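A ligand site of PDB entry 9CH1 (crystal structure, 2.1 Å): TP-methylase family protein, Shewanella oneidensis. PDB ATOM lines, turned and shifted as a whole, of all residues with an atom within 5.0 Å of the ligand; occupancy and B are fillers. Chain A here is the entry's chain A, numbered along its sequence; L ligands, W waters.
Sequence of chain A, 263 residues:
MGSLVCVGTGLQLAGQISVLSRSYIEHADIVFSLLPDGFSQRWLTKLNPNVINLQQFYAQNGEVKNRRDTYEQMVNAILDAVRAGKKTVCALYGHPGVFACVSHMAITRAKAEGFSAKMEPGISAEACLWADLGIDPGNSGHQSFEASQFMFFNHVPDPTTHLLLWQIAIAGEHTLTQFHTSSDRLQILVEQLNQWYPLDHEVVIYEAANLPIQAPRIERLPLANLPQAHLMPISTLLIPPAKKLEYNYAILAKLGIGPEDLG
The side-chain hydroxyl (OG1) of Thr 236 is in hydrogen-bond range of an oxygen (O5) of the ligand, 2.7 Å away.
The backbone NH (N) of Ala 208 lies within hydrogen-bond range of a nitrogen (N5) of the ligand (2.8 Å).
O of Ala 208 is in hydrogen-bond range of N4 of the ligand (3.0 Å).
The backbone carbonyl oxygen of Val 98 is in hydrogen-bond range of a nitrogen (N1) of the ligand, 2.8 Å away.
O4 of the ligand lies within hydrogen-bond range of O of Pro 233, 2.8 Å away.
The backbone NH of His 95 sits at hydrogen-bond distance from an oxygen (O1) of the ligand.
The backbone carbonyl oxygen (O) of His 95 is in hydrogen-bond range of a nitrogen (N1) of the ligand, 3.0 Å away.
O5 of the ligand sits at hydrogen-bond distance from N of Gln 167 (3.0 Å).
NE2 of Gln 167 lies close to S1 of the ligand (3.4 Å).
N of Ala 125 lies within hydrogen-bond range of O2 of the ligand.
N1 of the ligand lies within hydrogen-bond range of O of Tyr 93 (3.5 Å).
The backbone carbonyl oxygen of Ser 235 is in hydrogen-bond range of an oxygen (O5) of the ligand, at 3.3 Å.
The backbone carbonyl oxygen of Thr 236 sits at hydrogen-bond distance from the backbone NH of Tyr 206, 2.9 Å away.
OG of Ser 124 lies close to N of Glu 126 (3.5 Å).
The side-chain hydroxyl (OG) of Ser 235 sits at hydrogen-bond distance from the side-chain carboxylate (OE2) of Glu 207, at 2.5 Å.
OD1 of Asn 210 sits close to O of Leu 11, at 3.0 Å.
The backbone carbonyl oxygen (O) of Phe 99 lies close to a sulfur (S1) of the ligand (3.2 Å).
O of Ile 234 lies close to N6 of the ligand, 2.8 Å away.
CD1 of Leu 11 touches N4 of the ligand (3.4 Å).
CA of Gly 94 touches O1 of the ligand, at 3.6 Å.
Ser 124 touches the ligand.
CA of Trp 166 touches O5 of the ligand, at 3.4 Å.
Tyr 206 touches the ligand.
Glu 207 touches the ligand.
Hydrophobic or aromatic side chains within 4 Å of the ligand: Leu 11, Tyr 93, His 95, Val 98, Phe 99, Ala 125, Trp 166, Tyr 206, Ala 208 and Ile 234.
Of the 23 residues printed, 17 come within 4 Å of the ligand.
The nearest printed residue that does not touch the ligand is Asn 210 (4.1 Å).
Water W1 bridges N1 of the ligand (2.7 Å) and O of Tyr 93 (2.9 Å).
Water W3 lies within hydrogen-bond range of N4 of the ligand (3.0 Å) and OD1 of Asn 210 (3.0 Å).
Water W2 lies within hydrogen-bond range of the backbone carbonyl oxygen (O) of Ser 235, the backbone NH (N) of Ile 168, the backbone carbonyl oxygen (O) of Pro 233 and an oxygen (O4) of the ligand.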
ATOM      1  N   LEU A  11      29.369  19.324  -9.618  1.00  0.00           N
ATOM      2  CA  LEU A  11      29.357  20.717  -9.188  1.00  0.00           C
ATOM      3  C   LEU A  11      30.776  21.287  -9.213  1.00  0.00           C
ATOM      4  O   LEU A  11      30.977  22.423  -9.626  1.00  0.00           O
ATOM      5  CB  LEU A  11      28.750  20.817  -7.788  1.00  0.00           C
ATOM      6  CG  LEU A  11      27.217  20.810  -7.728  1.00  0.00           C
ATOM      7  CD1 LEU A  11      26.648  22.078  -8.329  1.00  0.00           C
ATOM      8  CD2 LEU A  11      26.669  19.583  -8.432  1.00  0.00           C
ATOM      9  N   TYR A  93      25.645  20.558 -15.744  1.00  0.00           N
ATOM     10  CA  TYR A  93      26.295  20.530 -14.439  1.00  0.00           C
ATOM     11  C   TYR A  93      25.450  19.685 -13.486  1.00  0.00           C
ATOM     12  O   TYR A  93      24.236  19.606 -13.624  1.00  0.00           O
ATOM     13  CB  TYR A  93      26.530  21.947 -13.894  1.00  0.00           C
ATOM     14  CG  TYR A  93      25.308  22.670 -13.345  1.00  0.00           C
ATOM     15  CD1 TYR A  93      24.860  22.437 -12.058  1.00  0.00           C
ATOM     16  CD2 TYR A  93      24.627  23.608 -14.119  1.00  0.00           C
ATOM     17  CE1 TYR A  93      23.744  23.099 -11.550  1.00  0.00           C
ATOM     18  CE2 TYR A  93      23.529  24.277 -13.624  1.00  0.00           C
ATOM     19  CZ  TYR A  93      23.077  24.023 -12.339  1.00  0.00           C
ATOM     20  OH  TYR A  93      21.988  24.681 -11.845  1.00  0.00           O
ATOM     21  N   GLY A  94      26.133  19.047 -12.525  1.00  0.00           N
ATOM     22  CA  GLY A  94      25.486  18.165 -11.579  1.00  0.00           C
ATOM     23  C   GLY A  94      25.018  16.869 -12.246  1.00  0.00           C
ATOM     24  O   GLY A  94      25.767  16.252 -13.001  1.00  0.00           O
ATOM     25  N   HIS A  95      23.770  16.485 -11.948  1.00  0.00           N
ATOM     26  CA  HIS A  95      23.118  15.340 -12.547  1.00  0.00           C
ATOM     27  C   HIS A  95      22.168  15.845 -13.633  1.00  0.00           C
ATOM     28  O   HIS A  95      21.336  16.713 -13.371  1.00  0.00           O
ATOM     29  CB  HIS A  95      22.423  14.525 -11.450  1.00  0.00           C
ATOM     30  CG  HIS A  95      21.727  13.280 -11.894  1.00  0.00           C
ATOM     31  ND1 HIS A  95      20.941  13.200 -13.024  1.00  0.00           N
ATOM     32  CD2 HIS A  95      21.657  12.077 -11.306  1.00  0.00           C
ATOM     33  CE1 HIS A  95      20.445  11.967 -13.118  1.00  0.00           C
ATOM     34  NE2 HIS A  95      20.873  11.269 -12.085  1.00  0.00           N
ATOM     35  N   VAL A  98      18.261  15.833 -12.932  1.00  0.00           N
ATOM     36  CA  VAL A  98      17.796  16.316 -11.634  1.00  0.00           C
ATOM     37  C   VAL A  98      17.466  17.802 -11.737  1.00  0.00           C
ATOM     38  O   VAL A  98      18.363  18.629 -11.883  1.00  0.00           O
ATOM     39  CB  VAL A  98      18.849  16.038 -10.539  1.00  0.00           C
ATOM     40  CG1 VAL A  98      18.502  16.731  -9.222  1.00  0.00           C
ATOM     41  CG2 VAL A  98      19.046  14.541 -10.320  1.00  0.00           C
ATOM     42  N   PHE A  99      16.169  18.114 -11.656  1.00  0.00           N
ATOM     43  CA  PHE A  99      15.675  19.482 -11.780  1.00  0.00           C
ATOM     44  C   PHE A  99      16.212  20.093 -13.077  1.00  0.00           C
ATOM     45  O   PHE A  99      16.739  21.196 -13.066  1.00  0.00           O
ATOM     46  CB  PHE A  99      16.078  20.294 -10.541  1.00  0.00           C
ATOM     47  CG  PHE A  99      15.290  19.945  -9.283  1.00  0.00           C
ATOM     48  CD1 PHE A  99      15.597  18.799  -8.559  1.00  0.00           C
ATOM     49  CD2 PHE A  99      14.263  20.758  -8.840  1.00  0.00           C
ATOM     50  CE1 PHE A  99      14.875  18.469  -7.418  1.00  0.00           C
ATOM     51  CE2 PHE A  99      13.546  20.431  -7.690  1.00  0.00           C
ATOM     52  CZ  PHE A  99      13.856  19.290  -6.983  1.00  0.00           C
ATOM     53  N   ALA A 100      16.052  19.354 -14.180  1.00  0.00           N
ATOM     54  CA  ALA A 100      16.568  19.756 -15.468  1.00  0.00           C
ATOM     55  C   ALA A 100      15.775  19.057 -16.567  1.00  0.00           C
ATOM     56  O   ALA A 100      15.905  17.850 -16.756  1.00  0.00           O
ATOM     57  CB  ALA A 100      18.044  19.449 -15.557  1.00  0.00           C
ATOM     58  N   ILE A 123      26.599  13.591 -10.246  1.00  0.00           N
ATOM     59  CA  ILE A 123      26.589  14.016  -8.855  1.00  0.00           C
ATOM     60  C   ILE A 123      25.864  15.350  -8.762  1.00  0.00           C
ATOM     61  O   ILE A 123      26.320  16.345  -9.323  1.00  0.00           O
ATOM     62  CB  ILE A 123      28.028  14.082  -8.314  1.00  0.00           C
ATOM     63  CG1 ILE A 123      28.691  12.701  -8.319  1.00  0.00           C
ATOM     64  CG2 ILE A 123      28.066  14.727  -6.928  1.00  0.00           C
ATOM     65  CD1 ILE A 123      30.189  12.732  -8.066  1.00  0.00           C
ATOM     66  N   SER A 124      24.734  15.365  -8.040  1.00  0.00           N
ATOM     67  CA  SER A 124      23.860  16.518  -7.969  1.00  0.00           C
ATOM     68  C   SER A 124      24.186  17.368  -6.734  1.00  0.00           C
ATOM     69  O   SER A 124      24.957  16.962  -5.878  1.00  0.00           O
ATOM     70  CB  SER A 124      22.410  16.101  -7.953  1.00  0.00           C
ATOM     71  OG  SER A 124      22.115  15.380  -6.771  1.00  0.00           O
ATOM     72  N   ALA A 125      23.536  18.533  -6.652  1.00  0.00           N
ATOM     73  CA  ALA A 125      23.711  19.442  -5.543  1.00  0.00           C
ATOM     74  C   ALA A 125      23.251  18.759  -4.253  1.00  0.00           C
ATOM     75  O   ALA A 125      23.816  18.978  -3.186  1.00  0.00           O
ATOM     76  CB  ALA A 125      22.944  20.720  -5.791  1.00  0.00           C
ATOM     77  N   GLU A 126      22.216  17.914  -4.382  1.00  0.00           N
ATOM     78  CA  GLU A 126      21.713  17.130  -3.275  1.00  0.00           C
ATOM     79  C   GLU A 126      22.807  16.211  -2.758  1.00  0.00           C
ATOM     80  O   GLU A 126      23.041  16.125  -1.554  1.00  0.00           O
ATOM     81  CB  GLU A 126      20.504  16.334  -3.764  1.00  0.00           C
ATOM     82  CG  GLU A 126      19.903  15.401  -2.719  1.00  0.00           C
ATOM     83  CD  GLU A 126      18.679  14.657  -3.205  1.00  0.00           C
ATOM     84  OE1 GLU A 126      17.667  15.325  -3.529  1.00  0.00           O
ATOM     85  OE2 GLU A 126      18.717  13.409  -3.279  1.00  0.00           O
ATOM     86  N   LEU A 165      14.187  22.578  -0.336  1.00  0.00           N
ATOM     87  CA  LEU A 165      13.477  23.391  -1.304  1.00  0.00           C
ATOM     88  C   LEU A 165      14.487  23.929  -2.321  1.00  0.00           C
ATOM     89  O   LEU A 165      15.340  24.743  -1.969  1.00  0.00           O
ATOM     90  CB  LEU A 165      12.719  24.525  -0.607  1.00  0.00           C
ATOM     91  CG  LEU A 165      11.625  24.089   0.376  1.00  0.00           C
ATOM     92  CD1 LEU A 165      10.812  25.299   0.826  1.00  0.00           C
ATOM     93  CD2 LEU A 165      10.724  23.033  -0.241  1.00  0.00           C
ATOM     94  N   TRP A 166      14.376  23.452  -3.565  1.00  0.00           N
ATOM     95  CA  TRP A 166      15.293  23.860  -4.617  1.00  0.00           C
ATOM     96  C   TRP A 166      14.807  25.159  -5.264  1.00  0.00           C
ATOM     97  O   TRP A 166      13.625  25.495  -5.186  1.00  0.00           O
ATOM     98  CB  TRP A 166      15.433  22.764  -5.690  1.00  0.00           C
ATOM     99  CG  TRP A 166      15.926  21.428  -5.191  1.00  0.00           C
ATOM    100  CD1 TRP A 166      15.418  20.682  -4.166  1.00  0.00           C
ATOM    101  CD2 TRP A 166      17.042  20.686  -5.721  1.00  0.00           C
ATOM    102  NE1 TRP A 166      16.132  19.526  -4.024  1.00  0.00           N
ATOM    103  CE2 TRP A 166      17.132  19.500  -4.966  1.00  0.00           C
ATOM    104  CE3 TRP A 166      17.955  20.901  -6.754  1.00  0.00           C
ATOM    105  CZ2 TRP A 166      18.118  18.537  -5.215  1.00  0.00           C
ATOM    106  CZ3 TRP A 166      18.924  19.949  -6.996  1.00  0.00           C
ATOM    107  CH2 TRP A 166      18.995  18.784  -6.238  1.00  0.00           C
ATOM    108  N   GLN A 167      15.732  25.874  -5.906  1.00  0.00           N
ATOM    109  CA  GLN A 167      15.409  27.085  -6.654  1.00  0.00           C
ATOM    110  C   GLN A 167      14.673  28.054  -5.747  1.00  0.00           C
ATOM    111  O   GLN A 167      13.677  28.671  -6.135  1.00  0.00           O
ATOM    112  CB  GLN A 167      14.627  26.703  -7.914  1.00  0.00           C
ATOM    113  CG  GLN A 167      15.470  25.945  -8.930  1.00  0.00           C
ATOM    114  CD  GLN A 167      14.695  25.527 -10.170  1.00  0.00           C
ATOM    115  OE1 GLN A 167      13.492  25.757 -10.297  1.00  0.00           O
ATOM    116  NE2 GLN A 167      15.409  24.898 -11.094  1.00  0.00           N
ATOM    117  N   ILE A 168      15.197  28.214  -4.528  1.00  0.00           N
ATOM    118  CA  ILE A 168      14.574  29.016  -3.498  1.00  0.00           C
ATOM    119  C   ILE A 168      14.679  30.496  -3.874  1.00  0.00           C
ATOM    120  O   ILE A 168      13.909  31.315  -3.378  1.00  0.00           O
ATOM    121  CB  ILE A 168      15.215  28.726  -2.124  1.00  0.00           C
ATOM    122  CG1 ILE A 168      14.539  29.495  -0.992  1.00  0.00           C
ATOM    123  CG2 ILE A 168      16.721  28.980  -2.166  1.00  0.00           C
ATOM    124  CD1 ILE A 168      13.097  29.073  -0.726  1.00  0.00           C
ATOM    125  N   TYR A 206      22.348  26.535   1.604  1.00  0.00           N
ATOM    126  CA  TYR A 206      23.483  25.748   1.163  1.00  0.00           C
ATOM    127  C   TYR A 206      23.823  26.073  -0.285  1.00  0.00           C
ATOM    128  O   TYR A 206      22.942  26.195  -1.128  1.00  0.00           O
ATOM    129  CB  TYR A 206      23.202  24.255   1.320  1.00  0.00           C
ATOM    130  CG  TYR A 206      24.267  23.355   0.692  1.00  0.00           C
ATOM    131  CD1 TYR A 206      25.521  23.218   1.276  1.00  0.00           C
ATOM    132  CD2 TYR A 206      24.018  22.644  -0.477  1.00  0.00           C
ATOM    133  CE1 TYR A 206      26.498  22.409   0.717  1.00  0.00           C
ATOM    134  CE2 TYR A 206      24.981  21.833  -1.040  1.00  0.00           C
ATOM    135  CZ  TYR A 206      26.230  21.710  -0.446  1.00  0.00           C
ATOM    136  OH  TYR A 206      27.176  20.911  -1.002  1.00  0.00           O
ATOM    137  N   GLU A 207      25.128  26.218  -0.548  1.00  0.00           N
ATOM    138  CA  GLU A 207      25.639  26.318  -1.900  1.00  0.00           C
ATOM    139  C   GLU A 207      26.934  25.509  -1.993  1.00  0.00           C
ATOM    140  O   GLU A 207      27.924  25.860  -1.360  1.00  0.00           O
ATOM    141  CB  GLU A 207      25.923  27.776  -2.299  1.00  0.00           C
ATOM    142  CG  GLU A 207      24.707  28.687  -2.190  1.00  0.00           C
ATOM    143  CD  GLU A 207      25.011  30.156  -2.425  1.00  0.00           C
ATOM    144  OE1 GLU A 207      26.181  30.473  -2.726  1.00  0.00           O
ATOM    145  OE2 GLU A 207      24.084  30.985  -2.310  1.00  0.00           O
ATOM    146  N   ALA A 208      26.901  24.421  -2.752  1.00  0.00           N
ATOM    147  CA  ALA A 208      28.097  23.639  -3.014  1.00  0.00           C
ATOM    148  C   ALA A 208      29.088  24.490  -3.800  1.00  0.00           C
ATOM    149  O   ALA A 208      28.699  25.293  -4.638  1.00  0.00           O
ATOM    150  CB  ALA A 208      27.745  22.373  -3.770  1.00  0.00           C
ATOM    151  N   ASN A 210      31.946  25.429  -6.538  1.00  0.00           N
ATOM    152  CA  ASN A 210      32.156  25.073  -7.936  1.00  0.00           C
ATOM    153  C   ASN A 210      33.658  24.997  -8.226  1.00  0.00           C
ATOM    154  O   ASN A 210      34.057  24.432  -9.242  1.00  0.00           O
ATOM    155  CB  ASN A 210      31.458  26.041  -8.879  1.00  0.00           C
ATOM    156  CG  ASN A 210      29.956  25.967  -8.767  1.00  0.00           C
ATOM    157  OD1 ASN A 210      29.363  24.921  -9.023  1.00  0.00           O
ATOM    158  ND2 ASN A 210      29.320  27.072  -8.408  1.00  0.00           N
ATOM    159  N   PRO A 233      20.929  32.127  -7.459  1.00  0.00           N
ATOM    160  CA  PRO A 233      20.329  31.058  -8.257  1.00  0.00           C
ATOM    161  C   PRO A 233      20.765  29.644  -7.868  1.00  0.00           C
ATOM    162  O   PRO A 233      20.007  28.698  -8.051  1.00  0.00           O
ATOM    163  CB  PRO A 233      20.777  31.415  -9.682  1.00  0.00           C
ATOM    164  CG  PRO A 233      20.910  32.919  -9.650  1.00  0.00           C
ATOM    165  CD  PRO A 233      21.505  33.201  -8.284  1.00  0.00           C
ATOM    166  N   ILE A 234      21.976  29.515  -7.322  1.00  0.00           N
ATOM    167  CA  ILE A 234      22.527  28.194  -7.018  1.00  0.00           C
ATOM    168  C   ILE A 234      22.179  27.790  -5.587  1.00  0.00           C
ATOM    169  O   ILE A 234      22.579  26.720  -5.135  1.00  0.00           O
ATOM    170  CB  ILE A 234      24.053  28.148  -7.248  1.00  0.00           C
ATOM    171  CG1 ILE A 234      24.797  29.161  -6.382  1.00  0.00           C
ATOM    172  CG2 ILE A 234      24.377  28.325  -8.734  1.00  0.00           C
ATOM    173  CD1 ILE A 234      26.289  28.912  -6.284  1.00  0.00           C
ATOM    174  N   SER A 235      21.423  28.633  -4.879  1.00  0.00           N
ATOM    175  CA  SER A 235      21.101  28.388  -3.479  1.00  0.00           C
ATOM    176  C   SER A 235      20.044  27.287  -3.353  1.00  0.00           C
ATOM    177  O   SER A 235      19.068  27.266  -4.105  1.00  0.00           O
ATOM    178  CB  SER A 235      20.644  29.638  -2.780  1.00  0.00           C
ATOM    179  OG  SER A 235      21.676  30.625  -2.733  1.00  0.00           O
ATOM    180  N   THR A 236      20.258  26.380  -2.391  1.00  0.00           N
ATOM    181  CA  THR A 236      19.247  25.431  -1.982  1.00  0.00           C
ATOM    182  C   THR A 236      18.969  25.639  -0.483  1.00  0.00           C
ATOM    183  O   THR A 236      19.891  25.873   0.288  1.00  0.00           O
ATOM    184  CB  THR A 236      19.714  24.010  -2.258  1.00  0.00           C
ATOM    185  OG1 THR A 236      19.775  23.894  -3.673  1.00  0.00           O
ATOM    186  CG2 THR A 236      18.776  22.958  -1.687  1.00  0.00           C
HETATM  187  N1  LIG L   1      20.994  19.501 -12.362  1.00  0.00           N
HETATM  188  C1  LIG L   1      21.350  20.318 -11.170  1.00  0.00           C
HETATM  189  C2  LIG L   1      20.149  21.136 -10.689  1.00  0.00           C
HETATM  190  C3  LIG L   1      19.869  22.365 -11.552  1.00  0.00           C
HETATM  191  S1  LIG L   1      18.335  23.213 -11.104  1.00  0.00           S
HETATM  192  C4  LIG L   1      21.828  19.376 -10.048  1.00  0.00           C
HETATM  193  O1  LIG L   1      22.064  18.195 -10.366  1.00  0.00           O
HETATM  194  O2  LIG L   1      21.952  19.853  -8.908  1.00  0.00           O
HETATM  195  C5  LIG L   1      19.053  24.620 -10.211  1.00  0.00           C
HETATM  196  C6  LIG L   1      18.914  24.422  -8.717  1.00  0.00           C
HETATM  197  O3  LIG L   1      19.823  23.387  -8.282  1.00  0.00           O
HETATM  198  C7  LIG L   1      19.259  25.619  -7.850  1.00  0.00           C
HETATM  199  O4  LIG L   1      18.184  26.544  -7.778  1.00  0.00           O
HETATM  200  C8  LIG L   1      19.549  24.914  -6.518  1.00  0.00           C
HETATM  201  O5  LIG L   1      18.372  24.523  -5.851  1.00  0.00           O
HETATM  202  C9  LIG L   1      20.337  23.708  -7.015  1.00  0.00           C
HETATM  203  N2  LIG L   1      21.766  23.985  -7.142  1.00  0.00           N
HETATM  204  C10 LIG L   1      22.453  24.233  -8.308  1.00  0.00           C
HETATM  205  N3  LIG L   1      23.720  24.469  -8.109  1.00  0.00           N
HETATM  206  C11 LIG L   1      23.885  24.401  -6.739  1.00  0.00           C
HETATM  207  C12 LIG L   1      25.005  24.559  -5.900  1.00  0.00           C
HETATM  208  N4  LIG L   1      26.218  24.842  -6.348  1.00  0.00           N
HETATM  209  N5  LIG L   1      24.813  24.415  -4.561  1.00  0.00           N
HETATM  210  C13 LIG L   1      23.586  24.130  -4.117  1.00  0.00           C
HETATM  211  N6  LIG L   1      22.460  23.954  -4.814  1.00  0.00           N
HETATM  212  C14 LIG L   1      22.676  24.105  -6.132  1.00  0.00           C
HETATM  213  O   HOH W   1      21.820  20.908 -14.466  1.00  0.00           O
HETATM  214  O   HOH W   2      17.898  29.176  -5.667  1.00  0.00           O
HETATM  215  O   HOH W   3      26.396  25.060  -9.290  1.00  0.00           O
